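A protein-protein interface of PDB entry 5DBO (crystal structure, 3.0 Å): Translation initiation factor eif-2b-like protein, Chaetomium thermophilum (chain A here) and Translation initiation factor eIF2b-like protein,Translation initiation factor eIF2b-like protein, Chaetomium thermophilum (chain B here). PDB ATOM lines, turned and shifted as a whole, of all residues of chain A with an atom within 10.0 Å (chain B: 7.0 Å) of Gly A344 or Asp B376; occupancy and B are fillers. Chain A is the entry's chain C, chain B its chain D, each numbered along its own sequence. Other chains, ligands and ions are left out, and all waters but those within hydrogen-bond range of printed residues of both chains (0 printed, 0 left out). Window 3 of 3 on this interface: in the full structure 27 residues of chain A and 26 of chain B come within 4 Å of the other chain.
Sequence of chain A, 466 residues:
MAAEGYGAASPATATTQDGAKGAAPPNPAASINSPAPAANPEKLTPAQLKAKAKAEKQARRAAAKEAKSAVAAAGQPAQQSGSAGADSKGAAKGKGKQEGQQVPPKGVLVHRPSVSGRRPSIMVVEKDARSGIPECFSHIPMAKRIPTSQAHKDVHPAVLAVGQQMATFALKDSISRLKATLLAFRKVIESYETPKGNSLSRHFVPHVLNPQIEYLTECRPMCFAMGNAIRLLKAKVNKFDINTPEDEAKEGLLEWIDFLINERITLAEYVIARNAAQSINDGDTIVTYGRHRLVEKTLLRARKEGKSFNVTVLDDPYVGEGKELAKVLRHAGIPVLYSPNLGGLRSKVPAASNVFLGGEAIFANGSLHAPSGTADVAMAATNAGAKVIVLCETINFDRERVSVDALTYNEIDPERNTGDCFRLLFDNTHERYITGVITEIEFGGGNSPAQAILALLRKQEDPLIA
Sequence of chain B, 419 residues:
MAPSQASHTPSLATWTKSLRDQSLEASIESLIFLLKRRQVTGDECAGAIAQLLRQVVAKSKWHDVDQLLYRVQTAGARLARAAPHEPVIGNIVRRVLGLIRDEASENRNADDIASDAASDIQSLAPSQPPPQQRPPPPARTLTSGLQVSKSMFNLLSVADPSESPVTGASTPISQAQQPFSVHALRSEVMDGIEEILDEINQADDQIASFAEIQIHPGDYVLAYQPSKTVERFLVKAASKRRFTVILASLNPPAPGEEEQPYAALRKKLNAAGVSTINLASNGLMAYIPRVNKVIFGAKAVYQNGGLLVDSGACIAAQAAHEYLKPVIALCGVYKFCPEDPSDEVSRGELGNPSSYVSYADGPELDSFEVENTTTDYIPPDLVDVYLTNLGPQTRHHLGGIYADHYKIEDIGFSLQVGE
The side-chain hydroxyl (OG) of Ser A347 is in hydrogen-bond range of the backbone NH (N) of Glu B349 (3.2 Å). The backbone NH (N) of Gly A344 lies within hydrogen-bond range of the side-chain carboxylate (OD2) of Asp B376 (2.7 Å).
The side-chain hydroxyl (OG1) of Thr B373 sits at hydrogen-bond distance from the side-chain carboxylate (OD1) of Asp B376. OD1 of Asn A341 lies within hydrogen-bond range of N of Gly A343 (2.8 Å). O of Asp B376 is in hydrogen-bond range of N of Val B309. OG of Ser A339 lies within hydrogen-bond range of O of Asn A341 (2.9 Å). The backbone NH (N) of Gly B312 lies within hydrogen-bond range of the side-chain carboxylate (OD2) of Asp B376, at 3.1 Å. O of Gly A344 lies close to OG of Ser A347 (3.3 Å).
Among the printed residues, merely in contact across the chains: Leu A342 with Ile B315 (3.3 Å), Ser A347 with Gly B348 (3.3 Å), Arg A346 with Cys B314 (3.7 Å), Gly A343 with Asp B376 (3.7 Å), Gly A343 with Gly B312 (3.9 Å) and Asn A341 with Leu B250 (3.97 Å).
Printed residues of chain B within 4 Å of Gly A343: Gly B312 and Asp B376. Gly A344 touches just one residue of chain B: Asp B376 (2.7 Å). Of the printed residues of chain B, Arg A346 touches Cys B314 (3.7 Å). No residue of chain A comes within 4 Å of Leu B308. No residue of chain A comes within 4 Å of Val B309. No residue of chain A comes within 4 Å of Ser B311. Gly B312 touches one residue of chain A. Printed residues of chain A within 4 Å of Cys B314: Arg A346 (3.7 Å). Of the printed residues of chain A, Ile B315 touches Leu A342 (3.3 Å). Asp B376 touches just these residues of chain A: Gly A343 (3.7 Å) and Gly A344 (2.7 Å). The nearest printed residue of chain A that does not touch Leu B250 is Gly A343 (4.1 Å).
Along chain A the printed residues that touch a printed residue of chain B span positions 341 to 347. Hydrophobic or aromatic side chains of chain B within 4 Å of the printed part of chain A: Leu B250 and Ile B315. Among the printed residues, 8 pairs touch across the chains.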
ATOM      1  N   VAL A 287     -14.523  -5.391   6.048  1.00  0.00           N
ATOM      2  CA  VAL A 287     -15.159  -5.039   7.306  1.00  0.00           C
ATOM      3  C   VAL A 287     -15.717  -3.626   7.219  1.00  0.00           C
ATOM      4  O   VAL A 287     -15.028  -2.707   6.776  1.00  0.00           O
ATOM      5  CB  VAL A 287     -14.173  -5.127   8.477  1.00  0.00           C
ATOM      6  CG1 VAL A 287     -14.900  -4.936   9.796  1.00  0.00           C
ATOM      7  CG2 VAL A 287     -13.466  -6.462   8.463  1.00  0.00           C
ATOM      8  N   THR A 312     -17.932  -8.477   6.707  1.00  0.00           N
ATOM      9  CA  THR A 312     -18.308  -8.427   8.109  1.00  0.00           C
ATOM     10  C   THR A 312     -18.879  -7.050   8.441  1.00  0.00           C
ATOM     11  O   THR A 312     -18.179  -6.036   8.369  1.00  0.00           O
ATOM     12  CB  THR A 312     -17.121  -8.706   9.025  1.00  0.00           C
ATOM     13  OG1 THR A 312     -16.556  -9.981   8.699  1.00  0.00           O
ATOM     14  CG2 THR A 312     -17.565  -8.685  10.485  1.00  0.00           C
ATOM     15  N   LEU A 314     -20.238  -4.566  11.172  1.00  0.00           N
ATOM     16  CA  LEU A 314     -20.292  -4.250  12.591  1.00  0.00           C
ATOM     17  C   LEU A 314     -21.368  -3.196  12.786  1.00  0.00           C
ATOM     18  O   LEU A 314     -21.669  -2.442  11.869  1.00  0.00           O
ATOM     19  CB  LEU A 314     -18.941  -3.745  13.095  1.00  0.00           C
ATOM     20  CG  LEU A 314     -17.787  -4.751  13.032  1.00  0.00           C
ATOM     21  CD1 LEU A 314     -16.470  -4.089  13.396  1.00  0.00           C
ATOM     22  CD2 LEU A 314     -18.053  -5.960  13.911  1.00  0.00           C
ATOM     23  N   TYR A 338     -22.649 -10.767  10.830  1.00  0.00           N
ATOM     24  CA  TYR A 338     -23.159  -9.581  11.502  1.00  0.00           C
ATOM     25  C   TYR A 338     -22.840  -9.557  12.994  1.00  0.00           C
ATOM     26  O   TYR A 338     -23.006 -10.552  13.688  1.00  0.00           O
ATOM     27  CB  TYR A 338     -24.670  -9.460  11.305  1.00  0.00           C
ATOM     28  CG  TYR A 338     -25.252  -8.254  12.008  1.00  0.00           C
ATOM     29  CD1 TYR A 338     -25.106  -6.978  11.475  1.00  0.00           C
ATOM     30  CD2 TYR A 338     -25.937  -8.390  13.206  1.00  0.00           C
ATOM     31  CE1 TYR A 338     -25.625  -5.872  12.120  1.00  0.00           C
ATOM     32  CE2 TYR A 338     -26.461  -7.291  13.855  1.00  0.00           C
ATOM     33  CZ  TYR A 338     -26.301  -6.034  13.309  1.00  0.00           C
ATOM     34  OH  TYR A 338     -26.830  -4.936  13.955  1.00  0.00           O
ATOM     35  N   SER A 339     -22.372  -8.405  13.469  1.00  0.00           N
ATOM     36  CA  SER A 339     -22.146  -8.179  14.891  1.00  0.00           C
ATOM     37  C   SER A 339     -22.906  -6.935  15.345  1.00  0.00           C
ATOM     38  O   SER A 339     -22.610  -5.823  14.907  1.00  0.00           O
ATOM     39  CB  SER A 339     -20.657  -8.027  15.188  1.00  0.00           C
ATOM     40  OG  SER A 339     -20.429  -7.930  16.583  1.00  0.00           O
ATOM     41  N   PRO A 340     -23.880  -7.118  16.245  1.00  0.00           N
ATOM     42  CA  PRO A 340     -24.780  -6.051  16.700  1.00  0.00           C
ATOM     43  C   PRO A 340     -24.061  -4.948  17.475  1.00  0.00           C
ATOM     44  O   PRO A 340     -24.628  -3.876  17.694  1.00  0.00           O
ATOM     45  CB  PRO A 340     -25.769  -6.794  17.599  1.00  0.00           C
ATOM     46  CG  PRO A 340     -24.998  -7.964  18.100  1.00  0.00           C
ATOM     47  CD  PRO A 340     -24.118  -8.382  16.961  1.00  0.00           C
ATOM     48  N   ASN A 341     -22.830  -5.223  17.890  1.00  0.00           N
ATOM     49  CA  ASN A 341     -22.049  -4.296  18.696  1.00  0.00           C
ATOM     50  C   ASN A 341     -20.566  -4.450  18.406  1.00  0.00           C
ATOM     51  O   ASN A 341     -20.177  -5.230  17.541  1.00  0.00           O
ATOM     52  CB  ASN A 341     -22.310  -4.525  20.181  1.00  0.00           C
ATOM     53  CG  ASN A 341     -22.126  -5.967  20.577  1.00  0.00           C
ATOM     54  OD1 ASN A 341     -21.008  -6.481  20.590  1.00  0.00           O
ATOM     55  ND2 ASN A 341     -23.227  -6.638  20.889  1.00  0.00           N
ATOM     56  N   LEU A 342     -19.744  -3.729  19.158  1.00  0.00           N
ATOM     57  CA  LEU A 342     -18.305  -3.719  18.930  1.00  0.00           C
ATOM     58  C   LEU A 342     -17.573  -4.663  19.872  1.00  0.00           C
ATOM     59  O   LEU A 342     -16.352  -4.599  19.991  1.00  0.00           O
ATOM     60  CB  LEU A 342     -17.763  -2.304  19.115  1.00  0.00           C
ATOM     61  CG  LEU A 342     -17.940  -1.337  17.947  1.00  0.00           C
ATOM     62  CD1 LEU A 342     -17.252  -0.017  18.274  1.00  0.00           C
ATOM     63  CD2 LEU A 342     -17.409  -1.938  16.661  1.00  0.00           C
ATOM     64  N   GLY A 343     -18.323  -5.528  20.549  1.00  0.00           N
ATOM     65  CA  GLY A 343     -17.728  -6.511  21.434  1.00  0.00           C
ATOM     66  C   GLY A 343     -16.966  -7.539  20.630  1.00  0.00           C
ATOM     67  O   GLY A 343     -17.344  -7.833  19.499  1.00  0.00           O
ATOM     68  N   GLY A 344     -15.889  -8.071  21.201  1.00  0.00           N
ATOM     69  CA  GLY A 344     -15.088  -9.082  20.533  1.00  0.00           C
ATOM     70  C   GLY A 344     -14.515  -8.570  19.228  1.00  0.00           C
ATOM     71  O   GLY A 344     -14.383  -9.312  18.257  1.00  0.00           O
ATOM     72  N   LEU A 345     -14.169  -7.290  19.220  1.00  0.00           N
ATOM     73  CA  LEU A 345     -13.701  -6.608  18.021  1.00  0.00           C
ATOM     74  C   LEU A 345     -12.421  -7.195  17.434  1.00  0.00           C
ATOM     75  O   LEU A 345     -12.307  -7.352  16.221  1.00  0.00           O
ATOM     76  CB  LEU A 345     -13.476  -5.129  18.336  1.00  0.00           C
ATOM     77  CG  LEU A 345     -13.288  -4.214  17.139  1.00  0.00           C
ATOM     78  CD1 LEU A 345     -14.382  -4.499  16.157  1.00  0.00           C
ATOM     79  CD2 LEU A 345     -13.340  -2.771  17.581  1.00  0.00           C
ATOM     80  N   ARG A 346     -11.466  -7.524  18.299  1.00  0.00           N
ATOM     81  CA  ARG A 346     -10.172  -8.038  17.865  1.00  0.00           C
ATOM     82  C   ARG A 346     -10.324  -9.317  17.052  1.00  0.00           C
ATOM     83  O   ARG A 346      -9.565  -9.573  16.116  1.00  0.00           O
ATOM     84  CB  ARG A 346      -9.260  -8.282  19.071  1.00  0.00           C
ATOM     85  CG  ARG A 346      -8.800  -7.004  19.768  1.00  0.00           C
ATOM     86  CD  ARG A 346      -7.943  -7.298  20.999  1.00  0.00           C
ATOM     87  NE  ARG A 346      -6.687  -7.969  20.670  1.00  0.00           N
ATOM     88  CZ  ARG A 346      -5.571  -7.340  20.309  1.00  0.00           C
ATOM     89  NH1 ARG A 346      -5.548  -6.017  20.225  1.00  0.00           N
ATOM     90  NH2 ARG A 346      -4.476  -8.035  20.029  1.00  0.00           N
ATOM     91  N   SER A 347     -11.323 -10.108  17.423  1.00  0.00           N
ATOM     92  CA  SER A 347     -11.616 -11.377  16.770  1.00  0.00           C
ATOM     93  C   SER A 347     -12.017 -11.205  15.319  1.00  0.00           C
ATOM     94  O   SER A 347     -11.585 -11.965  14.449  1.00  0.00           O
ATOM     95  CB  SER A 347     -12.737 -12.093  17.516  1.00  0.00           C
ATOM     96  OG  SER A 347     -12.546 -11.993  18.915  1.00  0.00           O
ATOM     97  N   LYS A 348     -12.849 -10.201  15.063  1.00  0.00           N
ATOM     98  CA  LYS A 348     -13.462 -10.045  13.752  1.00  0.00           C
ATOM     99  C   LYS A 348     -12.857  -8.934  12.900  1.00  0.00           C
ATOM    100  O   LYS A 348     -13.400  -8.586  11.850  1.00  0.00           O
ATOM    101  CB  LYS A 348     -14.973  -9.843  13.904  1.00  0.00           C
ATOM    102  CG  LYS A 348     -15.438  -9.364  15.256  1.00  0.00           C
ATOM    103  CD  LYS A 348     -16.875  -9.812  15.489  1.00  0.00           C
ATOM    104  CE  LYS A 348     -17.400  -9.312  16.818  1.00  0.00           C
ATOM    105  NZ  LYS A 348     -18.614 -10.042  17.285  1.00  0.00           N
ATOM    106  N   VAL A 349     -11.726  -8.392  13.338  1.00  0.00           N
ATOM    107  CA  VAL A 349     -10.926  -7.526  12.475  1.00  0.00           C
ATOM    108  C   VAL A 349      -9.507  -8.086  12.356  1.00  0.00           C
ATOM    109  O   VAL A 349      -8.569  -7.554  12.951  1.00  0.00           O
ATOM    110  CB  VAL A 349     -10.869  -6.080  12.999  1.00  0.00           C
ATOM    111  CG1 VAL A 349     -10.274  -5.168  11.948  1.00  0.00           C
ATOM    112  CG2 VAL A 349     -12.257  -5.596  13.375  1.00  0.00           C
ATOM    113  N   PRO A 350      -9.347  -9.179  11.593  1.00  0.00           N
ATOM    114  CA  PRO A 350      -8.028  -9.803  11.436  1.00  0.00           C
ATOM    115  C   PRO A 350      -7.089  -8.969  10.573  1.00  0.00           C
ATOM    116  O   PRO A 350      -7.545  -8.093   9.838  1.00  0.00           O
ATOM    117  CB  PRO A 350      -8.346 -11.137  10.744  1.00  0.00           C
ATOM    118  CG  PRO A 350      -9.839 -11.307  10.864  1.00  0.00           C
ATOM    119  CD  PRO A 350     -10.392  -9.926  10.875  1.00  0.00           C
ATOM    120  N   ASP A 376     -13.012   3.511  16.959  1.00  0.00           N
ATOM    121  CA  ASP A 376     -12.677   2.266  17.640  1.00  0.00           C
ATOM    122  C   ASP A 376     -12.346   1.181  16.620  1.00  0.00           C
ATOM    123  O   ASP A 376     -11.343   0.478  16.752  1.00  0.00           O
ATOM    124  CB  ASP A 376     -13.818   1.821  18.556  1.00  0.00           C
ATOM    125  CG  ASP A 376     -14.118   2.836  19.648  1.00  0.00           C
ATOM    126  OD1 ASP A 376     -13.620   2.665  20.783  1.00  0.00           O
ATOM    127  OD2 ASP A 376     -14.834   3.820  19.366  1.00  0.00           O
ATOM    128  N   VAL A 377     -13.189   1.048  15.601  1.00  0.00           N
ATOM    129  CA  VAL A 377     -12.954   0.065  14.550  1.00  0.00           C
ATOM    130  C   VAL A 377     -11.659   0.375  13.805  1.00  0.00           C
ATOM    131  O   VAL A 377     -10.853  -0.522  13.539  1.00  0.00           O
ATOM    132  CB  VAL A 377     -14.115   0.022  13.543  1.00  0.00           C
ATOM    133  CG1 VAL A 377     -13.862  -1.038  12.488  1.00  0.00           C
ATOM    134  CG2 VAL A 377     -15.426  -0.238  14.264  1.00  0.00           C
ATOM    135  N   ALA A 380      -8.643  -0.439  16.091  1.00  0.00           N
ATOM    136  CA  ALA A 380      -8.546  -1.880  16.246  1.00  0.00           C
ATOM    137  C   ALA A 380      -7.924  -2.490  14.996  1.00  0.00           C
ATOM    138  O   ALA A 380      -7.009  -3.322  15.074  1.00  0.00           O
ATOM    139  CB  ALA A 380      -9.916  -2.481  16.517  1.00  0.00           C
ATOM    140  N   LEU B 250     -21.896  -2.133  27.361  1.00  0.00           N
ATOM    141  CA  LEU B 250     -21.821  -2.591  25.975  1.00  0.00           C
ATOM    142  C   LEU B 250     -23.100  -2.341  25.195  1.00  0.00           C
ATOM    143  O   LEU B 250     -23.074  -1.821  24.081  1.00  0.00           O
ATOM    144  CB  LEU B 250     -21.515  -4.090  25.921  1.00  0.00           C
ATOM    145  CG  LEU B 250     -21.407  -4.681  24.510  1.00  0.00           C
ATOM    146  CD1 LEU B 250     -20.377  -3.938  23.671  1.00  0.00           C
ATOM    147  CD2 LEU B 250     -21.106  -6.162  24.546  1.00  0.00           C
ATOM    148  N   LEU B 307      -6.796 -11.585  30.582  1.00  0.00           N
ATOM    149  CA  LEU B 307      -8.033 -11.470  31.342  1.00  0.00           C
ATOM    150  C   LEU B 307      -9.230 -12.040  30.599  1.00  0.00           C
ATOM    151  O   LEU B 307      -9.298 -11.989  29.364  1.00  0.00           O
ATOM    152  CB  LEU B 307      -8.326 -10.007  31.690  1.00  0.00           C
ATOM    153  CG  LEU B 307      -7.309  -9.192  32.487  1.00  0.00           C
ATOM    154  CD1 LEU B 307      -7.885  -7.821  32.807  1.00  0.00           C
ATOM    155  CD2 LEU B 307      -6.915  -9.917  33.760  1.00  0.00           C
ATOM    156  N   LEU B 308     -10.161 -12.595  31.366  1.00  0.00           N
ATOM    157  CA  LEU B 308     -11.491 -12.884  30.859  1.00  0.00           C
ATOM    158  C   LEU B 308     -12.455 -11.850  31.436  1.00  0.00           C
ATOM    159  O   LEU B 308     -12.628 -11.761  32.652  1.00  0.00           O
ATOM    160  CB  LEU B 308     -11.922 -14.301  31.225  1.00  0.00           C
ATOM    161  CG  LEU B 308     -13.218 -14.777  30.571  1.00  0.00           C
ATOM    162  CD1 LEU B 308     -13.093 -14.730  29.060  1.00  0.00           C
ATOM    163  CD2 LEU B 308     -13.549 -16.182  31.043  1.00  0.00           C
ATOM    164  N   VAL B 309     -13.071 -11.063  30.561  1.00  0.00           N
ATOM    165  CA  VAL B 309     -13.909  -9.946  30.987  1.00  0.00           C
ATOM    166  C   VAL B 309     -15.280  -9.958  30.312  1.00  0.00           C
ATOM    167  O   VAL B 309     -15.574 -10.828  29.495  1.00  0.00           O
ATOM    168  CB  VAL B 309     -13.221  -8.607  30.691  1.00  0.00           C
ATOM    169  CG1 VAL B 309     -11.977  -8.449  31.545  1.00  0.00           C
ATOM    170  CG2 VAL B 309     -12.859  -8.522  29.221  1.00  0.00           C
ATOM    171  N   ASP B 310     -16.120  -8.989  30.654  1.00  0.00           N
ATOM    172  CA  ASP B 310     -17.395  -8.848  29.970  1.00  0.00           C
ATOM    173  C   ASP B 310     -17.127  -8.388  28.550  1.00  0.00           C
ATOM    174  O   ASP B 310     -16.105  -7.761  28.281  1.00  0.00           O
ATOM    175  CB  ASP B 310     -18.306  -7.852  30.687  1.00  0.00           C
ATOM    176  CG  ASP B 310     -18.302  -8.038  32.187  1.00  0.00           C
ATOM    177  OD1 ASP B 310     -18.991  -8.958  32.679  1.00  0.00           O
ATOM    178  OD2 ASP B 310     -17.601  -7.264  32.871  1.00  0.00           O
ATOM    179  N   SER B 311     -18.047  -8.691  27.645  1.00  0.00           N
ATOM    180  CA  SER B 311     -17.870  -8.327  26.253  1.00  0.00           C
ATOM    181  C   SER B 311     -17.876  -6.810  26.114  1.00  0.00           C
ATOM    182  O   SER B 311     -18.654  -6.119  26.771  1.00  0.00           O
ATOM    183  CB  SER B 311     -18.958  -8.957  25.387  1.00  0.00           C
ATOM    184  OG  SER B 311     -20.230  -8.801  25.988  1.00  0.00           O
ATOM    185  N   GLY B 312     -16.978  -6.294  25.283  1.00  0.00           N
ATOM    186  CA  GLY B 312     -16.898  -4.867  25.050  1.00  0.00           C
ATOM    187  C   GLY B 312     -15.958  -4.163  26.005  1.00  0.00           C
ATOM    188  O   GLY B 312     -15.662  -2.983  25.829  1.00  0.00           O
ATOM    189  N   ALA B 313     -15.484  -4.876  27.019  1.00  0.00           N
ATOM    190  CA  ALA B 313     -14.498  -4.306  27.929  1.00  0.00           C
ATOM    191  C   ALA B 313     -13.168  -4.086  27.214  1.00  0.00           C
ATOM    192  O   ALA B 313     -12.401  -3.177  27.550  1.00  0.00           O
ATOM    193  CB  ALA B 313     -14.305  -5.205  29.138  1.00  0.00           C
ATOM    194  N   CYS B 314     -12.907  -4.915  26.210  1.00  0.00           N
ATOM    195  CA  CYS B 314     -11.647  -4.849  25.493  1.00  0.00           C
ATOM    196  C   CYS B 314     -11.539  -3.569  24.659  1.00  0.00           C
ATOM    197  O   CYS B 314     -10.449  -3.039  24.484  1.00  0.00           O
ATOM    198  CB  CYS B 314     -11.481  -6.083  24.603  1.00  0.00           C
ATOM    199  SG  CYS B 314      -9.800  -6.350  24.002  1.00  0.00           S
ATOM    200  N   ILE B 315     -12.657  -3.053  24.161  1.00  0.00           N
ATOM    201  CA  ILE B 315     -12.595  -1.822  23.383  1.00  0.00           C
ATOM    202  C   ILE B 315     -12.200  -0.669  24.305  1.00  0.00           C
ATOM    203  O   ILE B 315     -11.439   0.227  23.918  1.00  0.00           O
ATOM    204  CB  ILE B 315     -13.930  -1.519  22.641  1.00  0.00           C
ATOM    205  CG1 ILE B 315     -14.981  -0.916  23.571  1.00  0.00           C
ATOM    206  CG2 ILE B 315     -14.463  -2.776  21.962  1.00  0.00           C
ATOM    207  CD1 ILE B 315     -16.329  -0.745  22.926  1.00  0.00           C
ATOM    208  N   VAL B 345      -9.380 -19.067  22.565  1.00  0.00           N
ATOM    209  CA  VAL B 345      -9.781 -17.945  23.391  1.00  0.00           C
ATOM    210  C   VAL B 345      -8.937 -16.744  23.003  1.00  0.00           C
ATOM    211  O   VAL B 345      -9.446 -15.634  22.859  1.00  0.00           O
ATOM    212  CB  VAL B 345      -9.568 -18.245  24.883  1.00  0.00           C
ATOM    213  CG1 VAL B 345      -9.964 -17.047  25.727  1.00  0.00           C
ATOM    214  CG2 VAL B 345     -10.358 -19.478  25.293  1.00  0.00           C
ATOM    215  N   GLY B 348      -9.989 -15.661  19.383  1.00  0.00           N
ATOM    216  CA  GLY B 348     -11.296 -15.034  19.369  1.00  0.00           C
ATOM    217  C   GLY B 348     -12.089 -15.314  20.627  1.00  0.00           C
ATOM    218  O   GLY B 348     -11.805 -16.269  21.346  1.00  0.00           O
ATOM    219  N   GLU B 349     -13.091 -14.483  20.888  1.00  0.00           N
ATOM    220  CA  GLU B 349     -13.934 -14.646  22.066  1.00  0.00           C
ATOM    221  C   GLU B 349     -14.704 -15.961  22.013  1.00  0.00           C
ATOM    222  O   GLU B 349     -14.142 -17.029  22.256  1.00  0.00           O
ATOM    223  N   THR B 373     -21.033 -13.142  21.930  1.00  0.00           N
ATOM    224  CA  THR B 373     -19.724 -13.491  22.470  1.00  0.00           C
ATOM    225  C   THR B 373     -19.805 -13.804  23.958  1.00  0.00           C
ATOM    226  O   THR B 373     -19.113 -14.692  24.451  1.00  0.00           O
ATOM    227  CB  THR B 373     -18.701 -12.366  22.244  1.00  0.00           C
ATOM    228  OG1 THR B 373     -17.451 -12.730  22.842  1.00  0.00           O
ATOM    229  CG2 THR B 373     -19.193 -11.066  22.862  1.00  0.00           C
ATOM    230  N   THR B 374     -20.656 -13.075  24.673  1.00  0.00           N
ATOM    231  CA  THR B 374     -20.819 -13.287  26.106  1.00  0.00           C
ATOM    232  C   THR B 374     -19.630 -12.751  26.900  1.00  0.00           C
ATOM    233  O   THR B 374     -19.798 -11.937  27.808  1.00  0.00           O
ATOM    234  CB  THR B 374     -21.029 -14.778  26.436  1.00  0.00           C
ATOM    235  OG1 THR B 374     -19.879 -15.532  26.034  1.00  0.00           O
ATOM    236  CG2 THR B 374     -22.255 -15.311  25.714  1.00  0.00           C
ATOM    237  N   THR B 375     -18.432 -13.213  26.558  1.00  0.00           N
ATOM    238  CA  THR B 375     -17.214 -12.782  27.236  1.00  0.00           C
ATOM    239  C   THR B 375     -16.114 -12.429  26.242  1.00  0.00           C
ATOM    240  O   THR B 375     -16.123 -12.895  25.106  1.00  0.00           O
ATOM    241  CB  THR B 375     -16.683 -13.854  28.202  1.00  0.00           C
ATOM    242  OG1 THR B 375     -16.289 -15.015  27.464  1.00  0.00           O
ATOM    243  CG2 THR B 375     -17.749 -14.237  29.210  1.00  0.00           C
ATOM    244  N   ASP B 376     -15.172 -11.602  26.678  1.00  0.00           N
ATOM    245  CA  ASP B 376     -14.061 -11.181  25.834  1.00  0.00           C
ATOM    246  C   ASP B 376     -12.728 -11.376  26.535  1.00  0.00           C
ATOM    247  O   ASP B 376     -12.651 -11.343  27.758  1.00  0.00           O
ATOM    248  CB  ASP B 376     -14.214  -9.716  25.428  1.00  0.00           C
ATOM    249  CG  ASP B 376     -15.130  -9.532  24.239  1.00  0.00           C
ATOM    250  OD1 ASP B 376     -15.688 -10.539  23.757  1.00  0.00           O
ATOM    251  OD2 ASP B 376     -15.287  -8.381  23.783  1.00  0.00           O
ATOM    252  N   TYR B 377     -11.679 -11.581  25.747  1.00  0.00           N
ATOM    253  CA  TYR B 377     -10.341 -11.783  26.281  1.00  0.00           C
ATOM    254  C   TYR B 377      -9.449 -10.564  26.075  1.00  0.00           C
ATOM    255  O   TYR B 377      -9.388 -10.003  24.987  1.00  0.00           O
ATOM    256  CB  TYR B 377      -9.698 -13.015  25.644  1.00  0.00           C
ATOM    257  CG  TYR B 377      -8.208 -13.124  25.872  1.00  0.00           C
ATOM    258  CD1 TYR B 377      -7.701 -13.755  26.997  1.00  0.00           C
ATOM    259  CD2 TYR B 377      -7.310 -12.594  24.961  1.00  0.00           C
ATOM    260  CE1 TYR B 377      -6.342 -13.854  27.206  1.00  0.00           C
ATOM    261  CE2 TYR B 377      -5.950 -12.691  25.162  1.00  0.00           C
ATOM    262  CZ  TYR B 377      -5.473 -13.320  26.286  1.00  0.00           C
ATOM    263  OH  TYR B 377      -4.119 -13.416  26.489  1.00  0.00           O
ATOM    264  N   ILE B 378      -8.756 -10.166  27.135  1.00  0.00           N
ATOM    265  CA  ILE B 378      -7.846  -9.025  27.088  1.00  0.00           C
ATOM    266  C   ILE B 378      -6.394  -9.459  27.292  1.00  0.00           C
ATOM    267  O   ILE B 378      -6.038  -9.929  28.369  1.00  0.00           O
ATOM    268  CB  ILE B 378      -8.198  -7.978  28.157  1.00  0.00           C
ATOM    269  CG1 ILE B 378      -9.621  -7.463  27.965  1.00  0.00           C
ATOM    270  CG2 ILE B 378      -7.202  -6.830  28.129  1.00  0.00           C
ATOM    271  CD1 ILE B 378      -9.969  -6.336  28.914  1.00  0.00           C
